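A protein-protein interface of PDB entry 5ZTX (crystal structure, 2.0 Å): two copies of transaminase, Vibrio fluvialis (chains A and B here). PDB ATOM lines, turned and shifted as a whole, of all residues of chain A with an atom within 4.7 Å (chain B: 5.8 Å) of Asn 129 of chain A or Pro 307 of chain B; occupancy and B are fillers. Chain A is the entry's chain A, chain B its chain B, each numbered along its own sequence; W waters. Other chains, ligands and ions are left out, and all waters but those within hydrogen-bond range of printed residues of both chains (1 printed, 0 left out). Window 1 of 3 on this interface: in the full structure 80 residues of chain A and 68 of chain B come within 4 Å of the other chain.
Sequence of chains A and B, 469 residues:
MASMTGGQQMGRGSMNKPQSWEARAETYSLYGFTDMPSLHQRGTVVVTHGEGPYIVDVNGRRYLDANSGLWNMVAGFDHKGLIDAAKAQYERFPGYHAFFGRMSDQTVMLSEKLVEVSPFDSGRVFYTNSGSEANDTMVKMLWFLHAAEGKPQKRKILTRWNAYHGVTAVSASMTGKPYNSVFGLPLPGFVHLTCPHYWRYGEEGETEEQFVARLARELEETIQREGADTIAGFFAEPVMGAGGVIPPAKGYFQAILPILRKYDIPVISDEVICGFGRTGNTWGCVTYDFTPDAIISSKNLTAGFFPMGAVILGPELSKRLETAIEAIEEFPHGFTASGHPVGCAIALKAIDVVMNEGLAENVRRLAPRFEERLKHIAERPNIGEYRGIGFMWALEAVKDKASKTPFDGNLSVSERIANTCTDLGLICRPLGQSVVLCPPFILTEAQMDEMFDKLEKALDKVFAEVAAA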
ATOM      1  N   THR A 128      17.074  17.001   9.536  1.00  0.00           N
ATOM      2  CA  THR A 128      18.316  16.775  10.201  1.00  0.00           C
ATOM      3  C   THR A 128      19.318  16.169   9.207  1.00  0.00           C
ATOM      4  O   THR A 128      19.034  16.050   8.030  1.00  0.00           O
ATOM      5  CB  THR A 128      18.149  15.813  11.330  1.00  0.00           C
ATOM      6  OG1 THR A 128      17.773  14.523  10.793  1.00  0.00           O
ATOM      7  CG2 THR A 128      17.052  16.231  12.249  1.00  0.00           C
ATOM      8  N   ASN A 129      20.503  15.825   9.692  1.00  0.00           N
ATOM      9  CA  ASN A 129      21.557  15.225   8.865  1.00  0.00           C
ATOM     10  C   ASN A 129      21.502  13.707   8.691  1.00  0.00           C
ATOM     11  O   ASN A 129      22.215  13.147   7.829  1.00  0.00           O
ATOM     12  CB  ASN A 129      22.899  15.613   9.422  1.00  0.00           C
ATOM     13  CG  ASN A 129      23.114  17.113   9.344  1.00  0.00           C
ATOM     14  OD1 ASN A 129      23.130  17.695   8.256  1.00  0.00           O
ATOM     15  ND2 ASN A 129      23.147  17.745  10.492  1.00  0.00           N
ATOM     16  N   SER A 130      20.660  13.055   9.479  1.00  0.00           N
ATOM     17  CA  SER A 130      20.607  11.589   9.536  1.00  0.00           C
ATOM     18  C   SER A 130      19.357  11.111  10.225  1.00  0.00           C
ATOM     19  O   SER A 130      18.720  11.850  10.959  1.00  0.00           O
ATOM     20  CB  SER A 130      21.787  11.053  10.371  1.00  0.00           C
ATOM     21  OG  SER A 130      21.711  11.448  11.776  1.00  0.00           O
ATOM     22  N   GLU A 133      19.784  11.475  14.028  1.00  0.00           N
ATOM     23  CA  GLU A 133      19.436  12.801  14.590  1.00  0.00           C
ATOM     24  C   GLU A 133      17.921  13.077  14.515  1.00  0.00           C
ATOM     25  O   GLU A 133      17.406  13.849  15.308  1.00  0.00           O
ATOM     26  CB  GLU A 133      20.088  13.953  13.861  1.00  0.00           C
ATOM     27  CG  GLU A 133      21.569  13.986  13.884  1.00  0.00           C
ATOM     28  CD  GLU A 133      22.140  15.353  13.407  1.00  0.00           C
ATOM     29  OE1 GLU A 133      21.499  16.064  12.527  1.00  0.00           O
ATOM     30  OE2 GLU A 133      23.264  15.640  13.894  1.00  0.00           O
ATOM     31  N   PHE A 306      22.723  11.892  -0.772  1.00  0.00           N
ATOM     32  CA  PHE A 306      23.068  12.967   0.152  1.00  0.00           C
ATOM     33  C   PHE A 306      22.614  12.570   1.617  1.00  0.00           C
ATOM     34  O   PHE A 306      21.501  12.090   1.811  1.00  0.00           O
ATOM     35  CB  PHE A 306      22.372  14.245  -0.251  1.00  0.00           C
ATOM     36  CG  PHE A 306      22.983  15.508   0.335  1.00  0.00           C
ATOM     37  CD1 PHE A 306      22.600  15.977   1.589  1.00  0.00           C
ATOM     38  CD2 PHE A 306      23.970  16.211  -0.390  1.00  0.00           C
ATOM     39  CE1 PHE A 306      23.146  17.127   2.123  1.00  0.00           C
ATOM     40  CE2 PHE A 306      24.529  17.375   0.138  1.00  0.00           C
ATOM     41  CZ  PHE A 306      24.106  17.835   1.408  1.00  0.00           C
ATOM     42  N   PRO A 307      23.446  12.818   2.610  1.00  0.00           N
ATOM     43  CA  PRO A 307      22.990  12.524   3.987  1.00  0.00           C
ATOM     44  C   PRO A 307      21.995  13.556   4.553  1.00  0.00           C
ATOM     45  O   PRO A 307      22.232  14.792   4.690  1.00  0.00           O
ATOM     46  CB  PRO A 307      24.299  12.402   4.802  1.00  0.00           C
ATOM     47  CG  PRO A 307      25.219  13.243   4.020  1.00  0.00           C
ATOM     48  CD  PRO A 307      24.856  13.187   2.560  1.00  0.00           C
ATOM     49  N   MET A 308      20.787  13.058   4.805  1.00  0.00           N
ATOM     50  CA  MET A 308      19.786  13.902   5.357  1.00  0.00           C
ATOM     51  C   MET A 308      18.700  13.055   5.995  1.00  0.00           C
ATOM     52  O   MET A 308      18.427  11.939   5.577  1.00  0.00           O
ATOM     53  CB  MET A 308      19.171  14.834   4.317  1.00  0.00           C
ATOM     54  CG  MET A 308      18.633  16.150   4.889  1.00  0.00           C
ATOM     55  SD  MET A 308      18.051  17.353   3.588  1.00  0.00           S
ATOM     56  CE  MET A 308      16.586  16.579   2.973  1.00  0.00           C
ATOM     57  N   GLY A 309      18.057  13.658   6.971  1.00  0.00           N
ATOM     58  CA  GLY A 309      16.847  13.087   7.653  1.00  0.00           C
ATOM     59  C   GLY A 309      15.732  14.102   7.570  1.00  0.00           C
ATOM     60  O   GLY A 309      15.999  15.344   7.406  1.00  0.00           O
ATOM     61  N   SER A 338      18.512  21.145  11.307  1.00  0.00           N
ATOM     62  CA  SER A 338      18.404  21.592   9.924  1.00  0.00           C
ATOM     63  C   SER A 338      19.013  20.510   9.010  1.00  0.00           C
ATOM     64  O   SER A 338      19.867  19.754   9.418  1.00  0.00           O
ATOM     65  CB  SER A 338      19.107  22.931   9.697  1.00  0.00           C
ATOM     66  OG  SER A 338      18.933  23.346   8.349  1.00  0.00           O
ATOM     67  N   GLY A 339      18.496  20.442   7.818  1.00  0.00           N
ATOM     68  CA  GLY A 339      19.005  19.620   6.735  1.00  0.00           C
ATOM     69  C   GLY A 339      20.028  20.355   5.919  1.00  0.00           C
ATOM     70  O   GLY A 339      21.113  20.736   6.465  1.00  0.00           O
ATOM     71  N   HIS A 340      19.748  20.485   4.619  1.00  0.00           N
ATOM     72  CA  HIS A 340      20.661  21.157   3.723  1.00  0.00           C
ATOM     73  C   HIS A 340      19.968  21.416   2.377  1.00  0.00           C
ATOM     74  O   HIS A 340      19.283  20.567   1.878  1.00  0.00           O
ATOM     75  CB  HIS A 340      21.871  20.256   3.525  1.00  0.00           C
ATOM     76  CG  HIS A 340      23.017  20.922   2.873  1.00  0.00           C
ATOM     77  ND1 HIS A 340      23.031  21.190   1.532  1.00  0.00           N
ATOM     78  CD2 HIS A 340      24.201  21.351   3.357  1.00  0.00           C
ATOM     79  CE1 HIS A 340      24.181  21.739   1.197  1.00  0.00           C
ATOM     80  NE2 HIS A 340      24.917  21.848   2.283  1.00  0.00           N
ATOM     81  N   THR B 128      31.370  11.392  11.188  1.00  0.00           N
ATOM     82  CA  THR B 128      29.944  11.450  11.408  1.00  0.00           C
ATOM     83  C   THR B 128      29.351  12.395  10.363  1.00  0.00           C
ATOM     84  O   THR B 128      30.070  12.939   9.479  1.00  0.00           O
ATOM     85  CB  THR B 128      29.641  11.984  12.815  1.00  0.00           C
ATOM     86  OG1 THR B 128      30.124  13.305  12.891  1.00  0.00           O
ATOM     87  CG2 THR B 128      30.323  11.127  13.907  1.00  0.00           C
ATOM     88  N   ASN B 129      28.051  12.605  10.465  1.00  0.00           N
ATOM     89  CA  ASN B 129      27.333  13.515   9.589  1.00  0.00           C
ATOM     90  C   ASN B 129      27.185  14.916  10.163  1.00  0.00           C
ATOM     91  O   ASN B 129      26.623  15.808   9.472  1.00  0.00           O
ATOM     92  CB  ASN B 129      25.962  12.981   9.247  1.00  0.00           C
ATOM     93  CG  ASN B 129      26.028  11.641   8.569  1.00  0.00           C
ATOM     94  OD1 ASN B 129      26.546  11.519   7.515  1.00  0.00           O
ATOM     95  ND2 ASN B 129      25.554  10.634   9.225  1.00  0.00           N
ATOM     96  N   SER B 130      27.664  15.150  11.387  1.00  0.00           N
ATOM     97  CA  SER B 130      27.580  16.487  11.983  1.00  0.00           C
ATOM     98  C   SER B 130      28.409  16.593  13.215  1.00  0.00           C
ATOM     99  O   SER B 130      28.702  15.587  13.831  1.00  0.00           O
ATOM    100  CB  SER B 130      26.163  16.834  12.426  1.00  0.00           C
ATOM    101  OG  SER B 130      25.765  15.952  13.458  1.00  0.00           O
ATOM    102  N   GLU B 133      26.685  14.836  16.098  1.00  0.00           N
ATOM    103  CA  GLU B 133      26.914  13.421  16.165  1.00  0.00           C
ATOM    104  C   GLU B 133      28.330  13.137  16.637  1.00  0.00           C
ATOM    105  O   GLU B 133      28.544  12.139  17.348  1.00  0.00           O
ATOM    106  CB  GLU B 133      26.675  12.692  14.856  1.00  0.00           C
ATOM    107  CG  GLU B 133      25.237  12.524  14.412  1.00  0.00           C
ATOM    108  CD  GLU B 133      25.140  11.986  12.958  1.00  0.00           C
ATOM    109  OE1 GLU B 133      26.117  11.308  12.439  1.00  0.00           O
ATOM    110  OE2 GLU B 133      24.109  12.327  12.312  1.00  0.00           O
ATOM    111  N   THR B 302      33.705  21.444   5.702  1.00  0.00           N
ATOM    112  CA  THR B 302      33.373  21.481   4.276  1.00  0.00           C
ATOM    113  C   THR B 302      32.885  22.865   3.892  1.00  0.00           C
ATOM    114  O   THR B 302      32.257  23.061   2.797  1.00  0.00           O
ATOM    115  CB  THR B 302      32.242  20.446   3.959  1.00  0.00           C
ATOM    116  OG1 THR B 302      31.116  20.778   4.753  1.00  0.00           O
ATOM    117  CG2 THR B 302      32.651  19.042   4.350  1.00  0.00           C
ATOM    118  N   PHE B 305      29.274  23.047   2.746  1.00  0.00           N
ATOM    119  CA  PHE B 305      28.849  22.428   1.477  1.00  0.00           C
ATOM    120  C   PHE B 305      28.329  21.024   1.641  1.00  0.00           C
ATOM    121  O   PHE B 305      27.742  20.491   0.718  1.00  0.00           O
ATOM    122  CB  PHE B 305      30.004  22.415   0.412  1.00  0.00           C
ATOM    123  CG  PHE B 305      30.140  23.724  -0.346  1.00  0.00           C
ATOM    124  CD1 PHE B 305      30.405  24.915   0.328  1.00  0.00           C
ATOM    125  CD2 PHE B 305      29.969  23.759  -1.713  1.00  0.00           C
ATOM    126  CE1 PHE B 305      30.502  26.134  -0.368  1.00  0.00           C
ATOM    127  CE2 PHE B 305      30.078  24.965  -2.432  1.00  0.00           C
ATOM    128  CZ  PHE B 305      30.329  26.173  -1.751  1.00  0.00           C
ATOM    129  N   PHE B 306      28.667  20.373   2.737  1.00  0.00           N
ATOM    130  CA  PHE B 306      28.335  18.979   2.903  1.00  0.00           C
ATOM    131  C   PHE B 306      28.356  18.566   4.387  1.00  0.00           C
ATOM    132  O   PHE B 306      29.328  18.844   5.108  1.00  0.00           O
ATOM    133  CB  PHE B 306      29.285  18.091   2.094  1.00  0.00           C
ATOM    134  CG  PHE B 306      28.815  16.672   1.883  1.00  0.00           C
ATOM    135  CD1 PHE B 306      28.995  15.707   2.842  1.00  0.00           C
ATOM    136  CD2 PHE B 306      28.199  16.301   0.684  1.00  0.00           C
ATOM    137  CE1 PHE B 306      28.609  14.362   2.588  1.00  0.00           C
ATOM    138  CE2 PHE B 306      27.742  15.004   0.461  1.00  0.00           C
ATOM    139  CZ  PHE B 306      27.951  14.029   1.393  1.00  0.00           C
ATOM    140  N   PRO B 307      27.309  17.859   4.816  1.00  0.00           N
ATOM    141  CA  PRO B 307      27.216  17.451   6.247  1.00  0.00           C
ATOM    142  C   PRO B 307      28.295  16.505   6.623  1.00  0.00           C
ATOM    143  O   PRO B 307      28.411  15.427   6.055  1.00  0.00           O
ATOM    144  CB  PRO B 307      25.865  16.761   6.379  1.00  0.00           C
ATOM    145  CG  PRO B 307      25.160  16.940   5.070  1.00  0.00           C
ATOM    146  CD  PRO B 307      26.081  17.565   4.046  1.00  0.00           C
ATOM    147  N   MET B 308      29.111  16.906   7.565  1.00  0.00           N
ATOM    148  CA  MET B 308      30.140  16.052   8.080  1.00  0.00           C
ATOM    149  C   MET B 308      30.519  16.512   9.457  1.00  0.00           C
ATOM    150  O   MET B 308      30.374  17.681   9.753  1.00  0.00           O
ATOM    151  CB  MET B 308      31.383  16.084   7.207  1.00  0.00           C
ATOM    152  CG  MET B 308      31.303  15.075   6.045  1.00  0.00           C
ATOM    153  SD  MET B 308      32.730  14.071   5.796  1.00  0.00           S
ATOM    154  CE  MET B 308      33.934  15.393   5.880  1.00  0.00           C
ATOM    155  N   GLY B 309      30.945  15.566  10.280  1.00  0.00           N
ATOM    156  CA  GLY B 309      31.693  15.845  11.509  1.00  0.00           C
ATOM    157  C   GLY B 309      32.855  14.916  11.660  1.00  0.00           C
ATOM    158  O   GLY B 309      32.964  13.901  10.941  1.00  0.00           O
ATOM    159  N   HIS B 340      32.123   9.880   4.602  1.00  0.00           N
ATOM    160  CA  HIS B 340      31.455   9.959   3.329  1.00  0.00           C
ATOM    161  C   HIS B 340      32.471  10.441   2.271  1.00  0.00           C
ATOM    162  O   HIS B 340      33.033  11.472   2.432  1.00  0.00           O
ATOM    163  CB  HIS B 340      30.284  10.913   3.392  1.00  0.00           C
ATOM    164  CG  HIS B 340      29.357  10.776   2.229  1.00  0.00           C
ATOM    165  ND1 HIS B 340      29.776  10.888   0.926  1.00  0.00           N
ATOM    166  CD2 HIS B 340      28.040  10.465   2.167  1.00  0.00           C
ATOM    167  CE1 HIS B 340      28.761  10.715   0.105  1.00  0.00           C
ATOM    168  NE2 HIS B 340      27.695  10.435   0.836  1.00  0.00           N
ATOM    169  N   GLY B 343      31.855  14.124   0.924  1.00  0.00           N
ATOM    170  CA  GLY B 343      32.230  14.995   2.026  1.00  0.00           C
ATOM    171  C   GLY B 343      33.747  15.135   2.210  1.00  0.00           C
ATOM    172  O   GLY B 343      34.231  16.227   2.487  1.00  0.00           O
HETATM  173  O   HOH W   1      23.823  14.634  16.563  1.00  0.00           O
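The side-chain carboxylate of Glu 133 of chain B is in hydrogen-bond range of the side-chain hydroxyl of Ser 130 of chain A (2.6 Å).
The side-chain hydroxyl (OG) of Ser 130 of chain B lies within hydrogen-bond range of the side-chain carboxylate (OE2) of Glu 133 of chain A, at 2.6 Å.
Among the printed residues, merely in contact across the chains: Asn 129 of chain A with Asn 129 of chain B (3.7 Å), Asn 129 of chain A with Ser 130 of chain B (3.7 Å), Asn 129 of chain A with Pro 307 of chain B (3.4 Å), Ser 130 of chain A with Asn 129 of chain B (3.96 Å), Glu 133 of chain A with Glu 133 of chain B (3.4 Å), Phe 306 of chain A with Phe 306 of chain B (3.9 Å), Phe 306 of chain A with Pro 307 of chain B (3.3 Å), Pro 307 of chain A with Asn 129 of chain B (3.6 Å), Pro 307 of chain A with Phe 306 of chain B (3.4 Å), Pro 307 of chain A with Pro 307 of chain B (3.7 Å) and His 340 of chain A with Phe 305 of chain B (3.5 Å).
Water W1 bridges N of Glu 133 of chain B (2.9 Å) and OE2 of Glu 133 of chain A (2.9 Å).
Of chain B, only Asn 129, Ser 130 and Pro 307 come within 4 Å of Asn 129 of chain A.
Of the printed residues of chain B, Glu 133 of chain A touches Ser 130 (2.6 Å) and Glu 133 (3.4 Å).
Thr 128 of chain B touches none of the printed residues of chain A.
Of the printed residues of chain A, Ser 130 of chain B touches Asn 129 and Glu 133.
Of the printed residues of chain A, Glu 133 of chain B touches Ser 130 and Glu 133.
Of the printed residues of chain A, Phe 305 of chain B touches His 340 (3.5 Å).
Printed residues of chain A within 4 Å of Phe 306 of chain B: Phe 306 (3.9 Å) and Pro 307 (3.4 Å).
Pro 307 of chain B touches just these residues of chain A: Asn 129, Phe 306 and Pro 307.
Gly 309 of chain B touches none of the printed residues of chain A.
The nearest residue of chain A that does not touch Pro 307 of chain B is His 340 of chain A (4.3 Å).
Asn 129 of chain A touches its own counterpart, Asn 129 of chain B.
Asn 129 of chain A touches Ser 130 of chain B, and with the chains exchanged Ser 130 of chain A touches Asn 129 of chain B.
Ser 130 of chain A touches Glu 133 of chain B, and with the chains exchanged Glu 133 of chain A touches Ser 130 of chain B.
Phe 306 of chain B touches its own counterpart, Phe 306 of chain A.
Of the 13 pairs that touch across the chains among the printed residues, 12 have their exchanged pair printed and touching as well.
The side-chain hydroxyl (OG) of Ser 130 of chain B is in hydrogen-bond range of the backbone NH (N) of Glu 133 of chain B (3.0 Å).
The side-chain hydroxyl (OG1) of Thr 128 of chain A lies within hydrogen-bond range of the backbone carbonyl oxygen (O) of Ser 130 of chain A (2.8 Å).
The backbone NH (N) of Asn 129 of chain B is in hydrogen-bond range of the side-chain carboxylate (OE1) of Glu 133 of chain B (3.1 Å).
The backbone carbonyl oxygen (O) of Ser 130 of chain B sits at hydrogen-bond distance from the side-chain hydroxyl (OG1) of Thr 128 of chain B (2.8 Å).
The side-chain sulfur of Met 308 of chain A is in hydrogen-bond range of the backbone NH of His 340 of chain A (3.7 Å).
The backbone carbonyl oxygen (O) of Phe 306 of chain B sits at hydrogen-bond distance from the side-chain hydroxyl (OG1) of Thr 302 of chain B (2.7 Å).
Hydrophobic or aromatic side chains of chain B that line the printed part of chain A: Phe 306 and Pro 307.
Hydrophobic or aromatic side chains of chain A that line the printed part of chain B: Phe 306, Pro 307 and His 340.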
